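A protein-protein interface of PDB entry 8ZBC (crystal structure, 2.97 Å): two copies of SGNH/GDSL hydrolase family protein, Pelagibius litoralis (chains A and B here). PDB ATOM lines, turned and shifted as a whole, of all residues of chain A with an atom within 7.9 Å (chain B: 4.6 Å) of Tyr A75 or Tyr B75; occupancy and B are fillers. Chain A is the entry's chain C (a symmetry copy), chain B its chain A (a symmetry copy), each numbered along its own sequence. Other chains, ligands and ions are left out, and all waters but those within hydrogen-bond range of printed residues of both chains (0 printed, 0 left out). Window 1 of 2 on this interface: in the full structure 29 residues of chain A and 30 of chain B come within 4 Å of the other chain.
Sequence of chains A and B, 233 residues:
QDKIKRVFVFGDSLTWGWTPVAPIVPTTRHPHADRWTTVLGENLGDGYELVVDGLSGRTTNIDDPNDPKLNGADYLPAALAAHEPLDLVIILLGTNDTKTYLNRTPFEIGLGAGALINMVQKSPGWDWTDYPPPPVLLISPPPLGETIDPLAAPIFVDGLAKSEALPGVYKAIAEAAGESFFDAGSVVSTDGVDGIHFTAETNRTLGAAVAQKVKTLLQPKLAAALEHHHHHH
The side-chain hydroxyl of Tyr B75 sits close to the side-chain hydroxyl of Tyr A75.
OD1 of Asp B53 lies within salt-bridge range of NH1 of Arg B58 (3.0 Å).
OD2 of Asp B53 lies within hydrogen-bond range of OH of Tyr B75.
The backbone carbonyl oxygen (O) of Asp A53 is in hydrogen-bond range of the backbone NH (N) of Gly A11 (3.0 Å).
The backbone carbonyl oxygen of Gly A11 lies within hydrogen-bond range of the backbone NH of Leu A55 (3.2 Å).
OD1 of Asp A53 is in salt-bridge range of NH1 of Arg A58 (3.0 Å).
OD2 of Asp A53 lies within hydrogen-bond range of OH of Tyr A75.
Among the printed residues, pairs that only touch across the chains: Val A52 with His B83 (3.7 Å), Asp A53 with His B83 (3.8 Å), Leu A55 with Ala B78 (3.7 Å), Lys A69 with Pro B77 (3.4 Å), Lys A69 with Ala B78 (3.6 Å), Tyr A75 with Ala B78 (3.6 Å), Tyr A75 with Ala B79 (3.4 Å), Ala A78 with Tyr B75 (3.4 Å), Ala A79 with Tyr B75 (3.4 Å) and Ala A82 with Asp B53 (3.8 Å).
Of the printed residues of chain B, Lys A69 touches Pro B77 (3.4 Å) and Ala B78 (3.6 Å).
Of chain B, only Tyr B75, Ala B78 and Ala B79 come within 4 Å of Tyr A75.
Asn B71 touches none of the printed residues of chain A.
Of the printed residues of chain A, Tyr B75 touches Tyr A75 (3.3 Å), Ala A78 (3.4 Å) and Ala A79 (3.4 Å).
Of the printed residues of chain A, Ala B78 touches Leu A55, Lys A69 and Tyr A75.
Of the printed residues of chain A, Ala B79 touches Tyr A75.
The nearest residue of chain A that does not touch Tyr B75 is Asp A53 (4.4 Å).
The nearest printed residue of chain B that does not touch Ala A79 is Asp B53 (5.5 Å).
Of the 26 printed residues of chain A, 8 touch a printed residue of chain B.
Hydrophobic or aromatic side chains of chain A that line the printed part of chain B: Leu A55, Tyr A75, Ala A78, Ala A79 and Ala A82.
Of the 13 printed residues of chain B, 6 touch a printed residue of chain A.
Among the printed residues, 11 pairs touch across the chains.
Asp A53 touches His B83, but with the chains exchanged His A83 does not touch Asp B53 (4.1 Å).
Tyr B75 touches its own counterpart, Tyr A75.
Tyr A75 touches Ala B78, and with the chains exchanged Ala A78 touches Tyr B75.
Tyr A75 touches Ala B79, and with the chains exchanged Ala A79 touches Tyr B75.
Positions printed for both chains: 10, 53, 58, 71, 72, 73, 74, 75, 76, 77, 78, 79 and 83.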
ATOM      1  N   PHE A   8     -30.352 -10.013 -22.979  1.00  0.00           N
ATOM      2  CA  PHE A   8     -30.632 -11.390 -23.370  1.00  0.00           C
ATOM      3  C   PHE A   8     -31.116 -12.172 -22.162  1.00  0.00           C
ATOM      4  O   PHE A   8     -30.448 -12.186 -21.125  1.00  0.00           O
ATOM      5  CB  PHE A   8     -29.371 -12.036 -23.930  1.00  0.00           C
ATOM      6  CG  PHE A   8     -29.549 -13.469 -24.343  1.00  0.00           C
ATOM      7  CD1 PHE A   8     -30.604 -13.854 -25.152  1.00  0.00           C
ATOM      8  CD2 PHE A   8     -28.643 -14.438 -23.935  1.00  0.00           C
ATOM      9  CE1 PHE A   8     -30.758 -15.166 -25.535  1.00  0.00           C
ATOM     10  CE2 PHE A   8     -28.797 -15.769 -24.314  1.00  0.00           C
ATOM     11  CZ  PHE A   8     -29.853 -16.131 -25.113  1.00  0.00           C
ATOM     12  N   PHE A  10     -32.142 -15.835 -20.664  1.00  0.00           N
ATOM     13  CA  PHE A  10     -31.871 -17.240 -20.912  1.00  0.00           C
ATOM     14  C   PHE A  10     -32.523 -18.038 -19.804  1.00  0.00           C
ATOM     15  O   PHE A  10     -32.101 -17.946 -18.644  1.00  0.00           O
ATOM     16  CB  PHE A  10     -30.358 -17.448 -20.899  1.00  0.00           C
ATOM     17  CG  PHE A  10     -29.923 -18.815 -21.348  1.00  0.00           C
ATOM     18  CD1 PHE A  10     -30.218 -19.263 -22.625  1.00  0.00           C
ATOM     19  CD2 PHE A  10     -29.186 -19.637 -20.504  1.00  0.00           C
ATOM     20  CE1 PHE A  10     -29.805 -20.510 -23.039  1.00  0.00           C
ATOM     21  CE2 PHE A  10     -28.773 -20.891 -20.918  1.00  0.00           C
ATOM     22  CZ  PHE A  10     -29.079 -21.327 -22.187  1.00  0.00           C
ATOM     23  N   GLY A  11     -33.551 -18.812 -20.137  1.00  0.00           N
ATOM     24  CA  GLY A  11     -34.277 -19.560 -19.112  1.00  0.00           C
ATOM     25  C   GLY A  11     -34.924 -20.841 -19.584  1.00  0.00           C
ATOM     26  O   GLY A  11     -34.564 -21.392 -20.608  1.00  0.00           O
ATOM     27  N   VAL A  52     -35.005 -13.160 -26.142  1.00  0.00           N
ATOM     28  CA  VAL A  52     -35.470 -14.142 -25.162  1.00  0.00           C
ATOM     29  C   VAL A  52     -35.279 -15.575 -25.638  1.00  0.00           C
ATOM     30  O   VAL A  52     -35.665 -15.927 -26.739  1.00  0.00           O
ATOM     31  CB  VAL A  52     -36.954 -13.903 -24.831  1.00  0.00           C
ATOM     32  CG1 VAL A  52     -37.443 -14.884 -23.769  1.00  0.00           C
ATOM     33  CG2 VAL A  52     -37.162 -12.463 -24.366  1.00  0.00           C
ATOM     34  N   ASP A  53     -34.683 -16.404 -24.788  1.00  0.00           N
ATOM     35  CA  ASP A  53     -34.502 -17.819 -25.109  1.00  0.00           C
ATOM     36  C   ASP A  53     -34.916 -18.690 -23.952  1.00  0.00           C
ATOM     37  O   ASP A  53     -34.116 -18.990 -23.082  1.00  0.00           O
ATOM     38  CB  ASP A  53     -33.054 -18.116 -25.513  1.00  0.00           C
ATOM     39  CG  ASP A  53     -32.951 -19.335 -26.393  1.00  0.00           C
ATOM     40  OD1 ASP A  53     -33.216 -20.439 -25.905  1.00  0.00           O
ATOM     41  OD2 ASP A  53     -32.627 -19.196 -27.586  1.00  0.00           O
ATOM     42  N   GLY A  54     -36.181 -19.093 -23.959  1.00  0.00           N
ATOM     43  CA  GLY A  54     -36.722 -19.988 -22.940  1.00  0.00           C
ATOM     44  C   GLY A  54     -37.072 -21.344 -23.504  1.00  0.00           C
ATOM     45  O   GLY A  54     -37.874 -21.440 -24.433  1.00  0.00           O
ATOM     46  N   LEU A  55     -36.468 -22.386 -22.943  1.00  0.00           N
ATOM     47  CA  LEU A  55     -36.697 -23.776 -23.379  1.00  0.00           C
ATOM     48  C   LEU A  55     -37.306 -24.597 -22.258  1.00  0.00           C
ATOM     49  O   LEU A  55     -36.685 -24.790 -21.224  1.00  0.00           O
ATOM     50  CB  LEU A  55     -35.378 -24.438 -23.822  1.00  0.00           C
ATOM     51  CG  LEU A  55     -35.424 -25.935 -24.186  1.00  0.00           C
ATOM     52  CD1 LEU A  55     -36.369 -26.176 -25.341  1.00  0.00           C
ATOM     53  CD2 LEU A  55     -34.045 -26.479 -24.518  1.00  0.00           C
ATOM     54  N   ARG A  58     -35.253 -27.098 -19.580  1.00  0.00           N
ATOM     55  CA  ARG A  58     -33.823 -26.784 -19.611  1.00  0.00           C
ATOM     56  C   ARG A  58     -33.179 -26.680 -18.220  1.00  0.00           C
ATOM     57  O   ARG A  58     -33.754 -26.084 -17.282  1.00  0.00           O
ATOM     58  CB  ARG A  58     -33.597 -25.496 -20.401  1.00  0.00           C
ATOM     59  CG  ARG A  58     -32.162 -24.953 -20.430  1.00  0.00           C
ATOM     60  CD  ARG A  58     -32.089 -23.615 -21.180  1.00  0.00           C
ATOM     61  NE  ARG A  58     -31.978 -23.781 -22.635  1.00  0.00           N
ATOM     62  CZ  ARG A  58     -32.288 -22.855 -23.546  1.00  0.00           C
ATOM     63  NH1 ARG A  58     -32.765 -21.669 -23.198  1.00  0.00           N
ATOM     64  NH2 ARG A  58     -32.125 -23.114 -24.827  1.00  0.00           N
ATOM     65  N   THR A  60     -29.345 -25.965 -15.908  1.00  0.00           N
ATOM     66  CA  THR A  60     -28.152 -25.143 -15.941  1.00  0.00           C
ATOM     67  C   THR A  60     -27.085 -25.759 -16.855  1.00  0.00           C
ATOM     68  O   THR A  60     -26.757 -25.194 -17.902  1.00  0.00           O
ATOM     69  CB  THR A  60     -27.526 -24.957 -14.550  1.00  0.00           C
ATOM     70  OG1 THR A  60     -27.340 -26.232 -13.922  1.00  0.00           O
ATOM     71  CG2 THR A  60     -28.398 -24.091 -13.677  1.00  0.00           C
ATOM     72  N   LYS A  69     -31.592 -32.318 -25.640  1.00  0.00           N
ATOM     73  CA  LYS A  69     -31.530 -30.868 -25.935  1.00  0.00           C
ATOM     74  C   LYS A  69     -31.695 -29.922 -24.746  1.00  0.00           C
ATOM     75  O   LYS A  69     -31.812 -28.724 -24.945  1.00  0.00           O
ATOM     76  CB  LYS A  69     -32.552 -30.496 -27.018  1.00  0.00           C
ATOM     77  CG  LYS A  69     -34.015 -30.516 -26.603  1.00  0.00           C
ATOM     78  CD  LYS A  69     -34.913 -30.299 -27.829  1.00  0.00           C
ATOM     79  CE  LYS A  69     -36.391 -30.317 -27.477  1.00  0.00           C
ATOM     80  NZ  LYS A  69     -36.937 -31.680 -27.310  1.00  0.00           N
ATOM     81  N   LEU A  70     -31.688 -30.454 -23.527  1.00  0.00           N
ATOM     82  CA  LEU A  70     -32.092 -29.703 -22.345  1.00  0.00           C
ATOM     83  C   LEU A  70     -30.949 -29.135 -21.497  1.00  0.00           C
ATOM     84  O   LEU A  70     -31.195 -28.549 -20.442  1.00  0.00           O
ATOM     85  CB  LEU A  70     -32.984 -30.566 -21.456  1.00  0.00           C
ATOM     86  CG  LEU A  70     -34.246 -31.100 -22.126  1.00  0.00           C
ATOM     87  CD1 LEU A  70     -35.075 -31.887 -21.118  1.00  0.00           C
ATOM     88  CD2 LEU A  70     -35.057 -29.960 -22.709  1.00  0.00           C
ATOM     89  N   ASN A  71     -29.717 -29.272 -21.951  1.00  0.00           N
ATOM     90  CA  ASN A  71     -28.585 -28.770 -21.194  1.00  0.00           C
ATOM     91  C   ASN A  71     -28.257 -27.340 -21.598  1.00  0.00           C
ATOM     92  O   ASN A  71     -27.726 -27.100 -22.686  1.00  0.00           O
ATOM     93  CB  ASN A  71     -27.383 -29.670 -21.437  1.00  0.00           C
ATOM     94  CG  ASN A  71     -26.252 -29.400 -20.485  1.00  0.00           C
ATOM     95  OD1 ASN A  71     -25.964 -28.245 -20.143  1.00  0.00           O
ATOM     96  ND2 ASN A  71     -25.587 -30.468 -20.056  1.00  0.00           N
ATOM     97  N   GLY A  72     -28.562 -26.388 -20.721  1.00  0.00           N
ATOM     98  CA  GLY A  72     -28.307 -24.963 -20.997  1.00  0.00           C
ATOM     99  C   GLY A  72     -26.898 -24.669 -21.492  1.00  0.00           C
ATOM    100  O   GLY A  72     -26.715 -23.885 -22.422  1.00  0.00           O
ATOM    101  N   ALA A  73     -25.907 -25.314 -20.879  1.00  0.00           N
ATOM    102  CA  ALA A  73     -24.506 -25.061 -21.182  1.00  0.00           C
ATOM    103  C   ALA A  73     -24.070 -25.613 -22.547  1.00  0.00           C
ATOM    104  O   ALA A  73     -23.084 -25.145 -23.122  1.00  0.00           O
ATOM    105  CB  ALA A  73     -23.642 -25.625 -20.069  1.00  0.00           C
ATOM    106  N   ASP A  74     -24.792 -26.605 -23.068  1.00  0.00           N
ATOM    107  CA  ASP A  74     -24.596 -27.031 -24.459  1.00  0.00           C
ATOM    108  C   ASP A  74     -24.934 -25.910 -25.446  1.00  0.00           C
ATOM    109  O   ASP A  74     -24.348 -25.833 -26.497  1.00  0.00           O
ATOM    110  CB  ASP A  74     -25.469 -28.248 -24.805  1.00  0.00           C
ATOM    111  CG  ASP A  74     -24.933 -29.558 -24.236  1.00  0.00           C
ATOM    112  OD1 ASP A  74     -23.776 -29.618 -23.827  1.00  0.00           O
ATOM    113  OD2 ASP A  74     -25.664 -30.558 -24.186  1.00  0.00           O
ATOM    114  N   TYR A  75     -25.883 -25.054 -25.093  1.00  0.00           N
ATOM    115  CA  TYR A  75     -26.488 -24.064 -26.004  1.00  0.00           C
ATOM    116  C   TYR A  75     -25.927 -22.643 -25.842  1.00  0.00           C
ATOM    117  O   TYR A  75     -25.820 -21.879 -26.832  1.00  0.00           O
ATOM    118  CB  TYR A  75     -27.982 -24.051 -25.694  1.00  0.00           C
ATOM    119  CG  TYR A  75     -28.956 -23.334 -26.608  1.00  0.00           C
ATOM    120  CD1 TYR A  75     -29.488 -23.959 -27.729  1.00  0.00           C
ATOM    121  CD2 TYR A  75     -29.452 -22.081 -26.271  1.00  0.00           C
ATOM    122  CE1 TYR A  75     -30.437 -23.325 -28.528  1.00  0.00           C
ATOM    123  CE2 TYR A  75     -30.393 -21.432 -27.060  1.00  0.00           C
ATOM    124  CZ  TYR A  75     -30.895 -22.070 -28.184  1.00  0.00           C
ATOM    125  OH  TYR A  75     -31.852 -21.459 -28.960  1.00  0.00           O
ATOM    126  N   LEU A  76     -25.567 -22.290 -24.607  1.00  0.00           N
ATOM    127  CA  LEU A  76     -25.324 -20.897 -24.273  1.00  0.00           C
ATOM    128  C   LEU A  76     -24.162 -20.237 -25.041  1.00  0.00           C
ATOM    129  O   LEU A  76     -24.307 -19.098 -25.478  1.00  0.00           O
ATOM    130  CB  LEU A  76     -25.151 -20.719 -22.763  1.00  0.00           C
ATOM    131  CG  LEU A  76     -25.044 -19.258 -22.289  1.00  0.00           C
ATOM    132  CD1 LEU A  76     -26.237 -18.438 -22.731  1.00  0.00           C
ATOM    133  CD2 LEU A  76     -24.890 -19.169 -20.786  1.00  0.00           C
ATOM    134  N   PRO A  77     -23.019 -20.934 -25.204  1.00  0.00           N
ATOM    135  CA  PRO A  77     -21.928 -20.327 -25.947  1.00  0.00           C
ATOM    136  C   PRO A  77     -22.351 -19.818 -27.323  1.00  0.00           C
ATOM    137  O   PRO A  77     -22.039 -18.665 -27.688  1.00  0.00           O
ATOM    138  CB  PRO A  77     -20.927 -21.478 -26.091  1.00  0.00           C
ATOM    139  CG  PRO A  77     -21.088 -22.201 -24.819  1.00  0.00           C
ATOM    140  CD  PRO A  77     -22.585 -22.211 -24.618  1.00  0.00           C
ATOM    141  N   ALA A  78     -23.078 -20.664 -28.063  1.00  0.00           N
ATOM    142  CA  ALA A  78     -23.549 -20.295 -29.386  1.00  0.00           C
ATOM    143  C   ALA A  78     -24.523 -19.126 -29.313  1.00  0.00           C
ATOM    144  O   ALA A  78     -24.433 -18.186 -30.088  1.00  0.00           O
ATOM    145  CB  ALA A  78     -24.197 -21.495 -30.065  1.00  0.00           C
ATOM    146  N   ALA A  79     -25.457 -19.202 -28.374  1.00  0.00           N
ATOM    147  CA  ALA A  79     -26.482 -18.182 -28.225  1.00  0.00           C
ATOM    148  C   ALA A  79     -25.861 -16.813 -27.968  1.00  0.00           C
ATOM    149  O   ALA A  79     -26.243 -15.822 -28.582  1.00  0.00           O
ATOM    150  CB  ALA A  79     -27.438 -18.571 -27.103  1.00  0.00           C
ATOM    151  N   LEU A  80     -24.889 -16.768 -27.071  1.00  0.00           N
ATOM    152  CA  LEU A  80     -24.231 -15.515 -26.715  1.00  0.00           C
ATOM    153  C   LEU A  80     -23.569 -14.836 -27.916  1.00  0.00           C
ATOM    154  O   LEU A  80     -23.689 -13.615 -28.088  1.00  0.00           O
ATOM    155  CB  LEU A  80     -23.179 -15.774 -25.642  1.00  0.00           C
ATOM    156  CG  LEU A  80     -23.692 -16.114 -24.252  1.00  0.00           C
ATOM    157  CD1 LEU A  80     -22.574 -16.723 -23.440  1.00  0.00           C
ATOM    158  CD2 LEU A  80     -24.278 -14.892 -23.557  1.00  0.00           C
ATOM    159  N   ALA A  81     -22.885 -15.644 -28.732  1.00  0.00           N
ATOM    160  CA  ALA A  81     -22.158 -15.164 -29.903  1.00  0.00           C
ATOM    161  C   ALA A  81     -23.105 -14.723 -31.011  1.00  0.00           C
ATOM    162  O   ALA A  81     -22.775 -13.854 -31.833  1.00  0.00           O
ATOM    163  CB  ALA A  81     -21.239 -16.251 -30.427  1.00  0.00           C
ATOM    164  N   ALA A  82     -24.270 -15.360 -31.036  1.00  0.00           N
ATOM    165  CA  ALA A  82     -25.289 -15.109 -32.037  1.00  0.00           C
ATOM    166  C   ALA A  82     -26.062 -13.819 -31.758  1.00  0.00           C
ATOM    167  O   ALA A  82     -26.702 -13.268 -32.674  1.00  0.00           O
ATOM    168  CB  ALA A  82     -26.245 -16.287 -32.106  1.00  0.00           C
ATOM    169  N   HIS A  83     -26.028 -13.359 -30.506  1.00  0.00           N
ATOM    170  CA  HIS A  83     -26.732 -12.141 -30.115  1.00  0.00           C
ATOM    171  C   HIS A  83     -25.807 -11.013 -29.652  1.00  0.00           C
ATOM    172  O   HIS A  83     -26.283  -9.949 -29.256  1.00  0.00           O
ATOM    173  CB  HIS A  83     -27.770 -12.470 -29.055  1.00  0.00           C
ATOM    174  CG  HIS A  83     -28.737 -13.523 -29.487  1.00  0.00           C
ATOM    175  ND1 HIS A  83     -29.423 -13.448 -30.673  1.00  0.00           N
ATOM    176  CD2 HIS A  83     -29.129 -14.677 -28.898  1.00  0.00           C
ATOM    177  CE1 HIS A  83     -30.196 -14.513 -30.801  1.00  0.00           C
ATOM    178  NE2 HIS A  83     -30.032 -15.277 -29.736  1.00  0.00           N
ATOM    179  N   LEU A 116     -22.425 -21.363 -16.364  1.00  0.00           N
ATOM    180  CA  LEU A 116     -23.039 -20.499 -17.365  1.00  0.00           C
ATOM    181  C   LEU A 116     -22.489 -19.074 -17.269  1.00  0.00           C
ATOM    182  O   LEU A 116     -22.189 -18.461 -18.279  1.00  0.00           O
ATOM    183  CB  LEU A 116     -24.569 -20.512 -17.233  1.00  0.00           C
ATOM    184  CG  LEU A 116     -25.254 -21.867 -17.458  1.00  0.00           C
ATOM    185  CD1 LEU A 116     -26.755 -21.761 -17.240  1.00  0.00           C
ATOM    186  CD2 LEU A 116     -24.941 -22.412 -18.839  1.00  0.00           C
ATOM    187  N   MET A 119     -19.230 -19.006 -18.956  1.00  0.00           N
ATOM    188  CA  MET A 119     -19.376 -18.974 -20.414  1.00  0.00           C
ATOM    189  C   MET A 119     -19.649 -17.551 -20.924  1.00  0.00           C
ATOM    190  O   MET A 119     -19.124 -17.156 -21.965  1.00  0.00           O
ATOM    191  CB  MET A 119     -20.471 -19.932 -20.874  1.00  0.00           C
ATOM    192  CG  MET A 119     -20.049 -21.375 -20.828  1.00  0.00           C
ATOM    193  SD  MET A 119     -21.442 -22.501 -20.995  1.00  0.00           S
ATOM    194  CE  MET A 119     -20.575 -23.995 -21.511  1.00  0.00           C
ATOM    195  N   PHE B  10     -32.589 -19.364 -39.235  1.00  0.00           N
ATOM    196  CA  PHE B  10     -31.468 -20.071 -38.625  1.00  0.00           C
ATOM    197  C   PHE B  10     -30.311 -20.009 -39.600  1.00  0.00           C
ATOM    198  O   PHE B  10     -30.375 -20.601 -40.666  1.00  0.00           O
ATOM    199  CB  PHE B  10     -31.883 -21.522 -38.370  1.00  0.00           C
ATOM    200  CG  PHE B  10     -30.906 -22.306 -37.561  1.00  0.00           C
ATOM    201  CD1 PHE B  10     -30.592 -21.921 -36.277  1.00  0.00           C
ATOM    202  CD2 PHE B  10     -30.317 -23.453 -38.076  1.00  0.00           C
ATOM    203  CE1 PHE B  10     -29.703 -22.656 -35.520  1.00  0.00           C
ATOM    204  CE2 PHE B  10     -29.418 -24.193 -37.326  1.00  0.00           C
ATOM    205  CZ  PHE B  10     -29.113 -23.792 -36.050  1.00  0.00           C
ATOM    206  N   ASP B  53     -31.726 -16.350 -35.511  1.00  0.00           N
ATOM    207  CA  ASP B  53     -30.585 -16.947 -34.830  1.00  0.00           C
ATOM    208  C   ASP B  53     -29.444 -17.152 -35.804  1.00  0.00           C
ATOM    209  O   ASP B  53     -29.346 -18.194 -36.450  1.00  0.00           O
ATOM    210  CB  ASP B  53     -30.959 -18.271 -34.176  1.00  0.00           C
ATOM    211  CG  ASP B  53     -30.029 -18.629 -33.028  1.00  0.00           C
ATOM    212  OD1 ASP B  53     -28.826 -18.874 -33.275  1.00  0.00           O
ATOM    213  OD2 ASP B  53     -30.512 -18.679 -31.882  1.00  0.00           O
ATOM    214  N   ARG B  58     -21.025 -20.805 -38.127  1.00  0.00           N
ATOM    215  CA  ARG B  58     -21.892 -21.980 -37.983  1.00  0.00           C
ATOM    216  C   ARG B  58     -22.007 -22.848 -39.242  1.00  0.00           C
ATOM    217  O   ARG B  58     -22.156 -22.336 -40.367  1.00  0.00           O
ATOM    218  CB  ARG B  58     -23.295 -21.546 -37.520  1.00  0.00           C
ATOM    219  CG  ARG B  58     -24.328 -22.665 -37.365  1.00  0.00           C
ATOM    220  CD  ARG B  58     -25.691 -22.097 -36.940  1.00  0.00           C
ATOM    221  NE  ARG B  58     -25.818 -21.936 -35.495  1.00  0.00           N
ATOM    222  CZ  ARG B  58     -26.677 -21.127 -34.875  1.00  0.00           C
ATOM    223  NH1 ARG B  58     -27.499 -20.346 -35.549  1.00  0.00           N
ATOM    224  NH2 ARG B  58     -26.701 -21.092 -33.557  1.00  0.00           N
ATOM    225  N   ASN B  71     -21.617 -26.048 -34.511  1.00  0.00           N
ATOM    226  CA  ASN B  71     -22.388 -27.066 -35.183  1.00  0.00           C
ATOM    227  C   ASN B  71     -23.882 -26.775 -35.077  1.00  0.00           C
ATOM    228  O   ASN B  71     -24.479 -26.932 -34.013  1.00  0.00           O
ATOM    229  CB  ASN B  71     -22.081 -28.417 -34.570  1.00  0.00           C
ATOM    230  CG  ASN B  71     -22.619 -29.569 -35.381  1.00  0.00           C
ATOM    231  OD1 ASN B  71     -23.718 -29.501 -35.937  1.00  0.00           O
ATOM    232  ND2 ASN B  71     -21.848 -30.645 -35.440  1.00  0.00           N
ATOM    233  N   GLY B  72     -24.489 -26.364 -36.196  1.00  0.00           N
ATOM    234  CA  GLY B  72     -25.925 -26.043 -36.235  1.00  0.00           C
ATOM    235  C   GLY B  72     -26.817 -27.100 -35.616  1.00  0.00           C
ATOM    236  O   GLY B  72     -27.744 -26.784 -34.882  1.00  0.00           O
ATOM    237  N   ALA B  73     -26.520 -28.363 -35.906  1.00  0.00           N
ATOM    238  CA  ALA B  73     -27.348 -29.487 -35.473  1.00  0.00           C
ATOM    239  C   ALA B  73     -27.229 -29.771 -33.972  1.00  0.00           C
ATOM    240  O   ALA B  73     -28.137 -30.373 -33.385  1.00  0.00           O
ATOM    241  CB  ALA B  73     -26.998 -30.713 -36.283  1.00  0.00           C
ATOM    242  N   ASP B  74     -26.128 -29.350 -33.340  1.00  0.00           N
ATOM    243  CA  ASP B  74     -26.043 -29.370 -31.877  1.00  0.00           C
ATOM    244  C   ASP B  74     -27.087 -28.455 -31.236  1.00  0.00           C
ATOM    245  O   ASP B  74     -27.568 -28.733 -30.162  1.00  0.00           O
ATOM    246  CB  ASP B  74     -24.659 -28.917 -31.383  1.00  0.00           C
ATOM    247  CG  ASP B  74     -23.579 -29.978 -31.537  1.00  0.00           C
ATOM    248  OD1 ASP B  74     -23.905 -31.152 -31.704  1.00  0.00           O
ATOM    249  OD2 ASP B  74     -22.388 -29.630 -31.467  1.00  0.00           O
ATOM    250  N   TYR B  75     -27.426 -27.367 -31.911  1.00  0.00           N
ATOM    251  CA  TYR B  75     -28.225 -26.260 -31.358  1.00  0.00           C
ATOM    252  C   TYR B  75     -29.703 -26.289 -31.769  1.00  0.00           C
ATOM    253  O   TYR B  75     -30.577 -25.887 -31.001  1.00  0.00           O
ATOM    254  CB  TYR B  75     -27.576 -24.977 -31.875  1.00  0.00           C
ATOM    255  CG  TYR B  75     -27.980 -23.636 -31.300  1.00  0.00           C
ATOM    256  CD1 TYR B  75     -29.039 -22.924 -31.849  1.00  0.00           C
ATOM    257  CD2 TYR B  75     -27.216 -23.010 -30.309  1.00  0.00           C
ATOM    258  CE1 TYR B  75     -29.370 -21.651 -31.380  1.00  0.00           C
ATOM    259  CE2 TYR B  75     -27.540 -21.748 -29.835  1.00  0.00           C
ATOM    260  CZ  TYR B  75     -28.609 -21.067 -30.373  1.00  0.00           C
ATOM    261  OH  TYR B  75     -28.927 -19.813 -29.916  1.00  0.00           O
ATOM    262  N   LEU B  76     -29.977 -26.772 -32.976  1.00  0.00           N
ATOM    263  CA  LEU B  76     -31.282 -26.568 -33.591  1.00  0.00           C
ATOM    264  C   LEU B  76     -32.450 -27.210 -32.836  1.00  0.00           C
ATOM    265  O   LEU B  76     -33.492 -26.569 -32.697  1.00  0.00           O
ATOM    266  CB  LEU B  76     -31.276 -27.013 -35.063  1.00  0.00           C
ATOM    267  CG  LEU B  76     -32.570 -26.701 -35.838  1.00  0.00           C
ATOM    268  CD1 LEU B  76     -32.923 -25.222 -35.786  1.00  0.00           C
ATOM    269  CD2 LEU B  76     -32.458 -27.153 -37.272  1.00  0.00           C
ATOM    270  N   PRO B  77     -32.296 -28.462 -32.345  1.00  0.00           N
ATOM    271  CA  PRO B  77     -33.403 -29.056 -31.602  1.00  0.00           C
ATOM    272  C   PRO B  77     -33.895 -28.170 -30.456  1.00  0.00           C
ATOM    273  O   PRO B  77     -35.110 -27.950 -30.308  1.00  0.00           O
ATOM    274  CB  PRO B  77     -32.809 -30.360 -31.079  1.00  0.00           C
ATOM    275  CG  PRO B  77     -31.874 -30.748 -32.152  1.00  0.00           C
ATOM    276  CD  PRO B  77     -31.227 -29.445 -32.557  1.00  0.00           C
ATOM    277  N   ALA B  78     -32.956 -27.654 -29.669  1.00  0.00           N
ATOM    278  CA  ALA B  78     -33.287 -26.772 -28.556  1.00  0.00           C
ATOM    279  C   ALA B  78     -33.929 -25.484 -29.048  1.00  0.00           C
ATOM    280  O   ALA B  78     -34.921 -25.040 -28.503  1.00  0.00           O
ATOM    281  CB  ALA B  78     -32.036 -26.468 -27.733  1.00  0.00           C
ATOM    282  N   ALA B  79     -33.354 -24.892 -30.079  1.00  0.00           N
ATOM    283  CA  ALA B  79     -33.849 -23.628 -30.619  1.00  0.00           C
ATOM    284  C   ALA B  79     -35.297 -23.755 -31.084  1.00  0.00           C
ATOM    285  O   ALA B  79     -36.128 -22.899 -30.769  1.00  0.00           O
ATOM    286  CB  ALA B  79     -32.960 -23.170 -31.757  1.00  0.00           C
ATOM    287  N   HIS B  83     -38.704 -21.757 -29.400  1.00  0.00           N
ATOM    288  CA  HIS B  83     -39.480 -20.773 -30.150  1.00  0.00           C
ATOM    289  C   HIS B  83     -40.806 -21.312 -30.687  1.00  0.00           C
ATOM    290  O   HIS B  83     -41.523 -20.600 -31.384  1.00  0.00           O
ATOM    291  CB  HIS B  83     -38.618 -20.201 -31.262  1.00  0.00           C
ATOM    292  CG  HIS B  83     -37.343 -19.600 -30.765  1.00  0.00           C
ATOM    293  ND1 HIS B  83     -37.313 -18.672 -29.747  1.00  0.00           N
ATOM    294  CD2 HIS B  83     -36.056 -19.797 -31.136  1.00  0.00           C
ATOM    295  CE1 HIS B  83     -36.062 -18.312 -29.525  1.00  0.00           C
ATOM    296  NE2 HIS B  83     -35.280 -18.983 -30.353  1.00  0.00           N
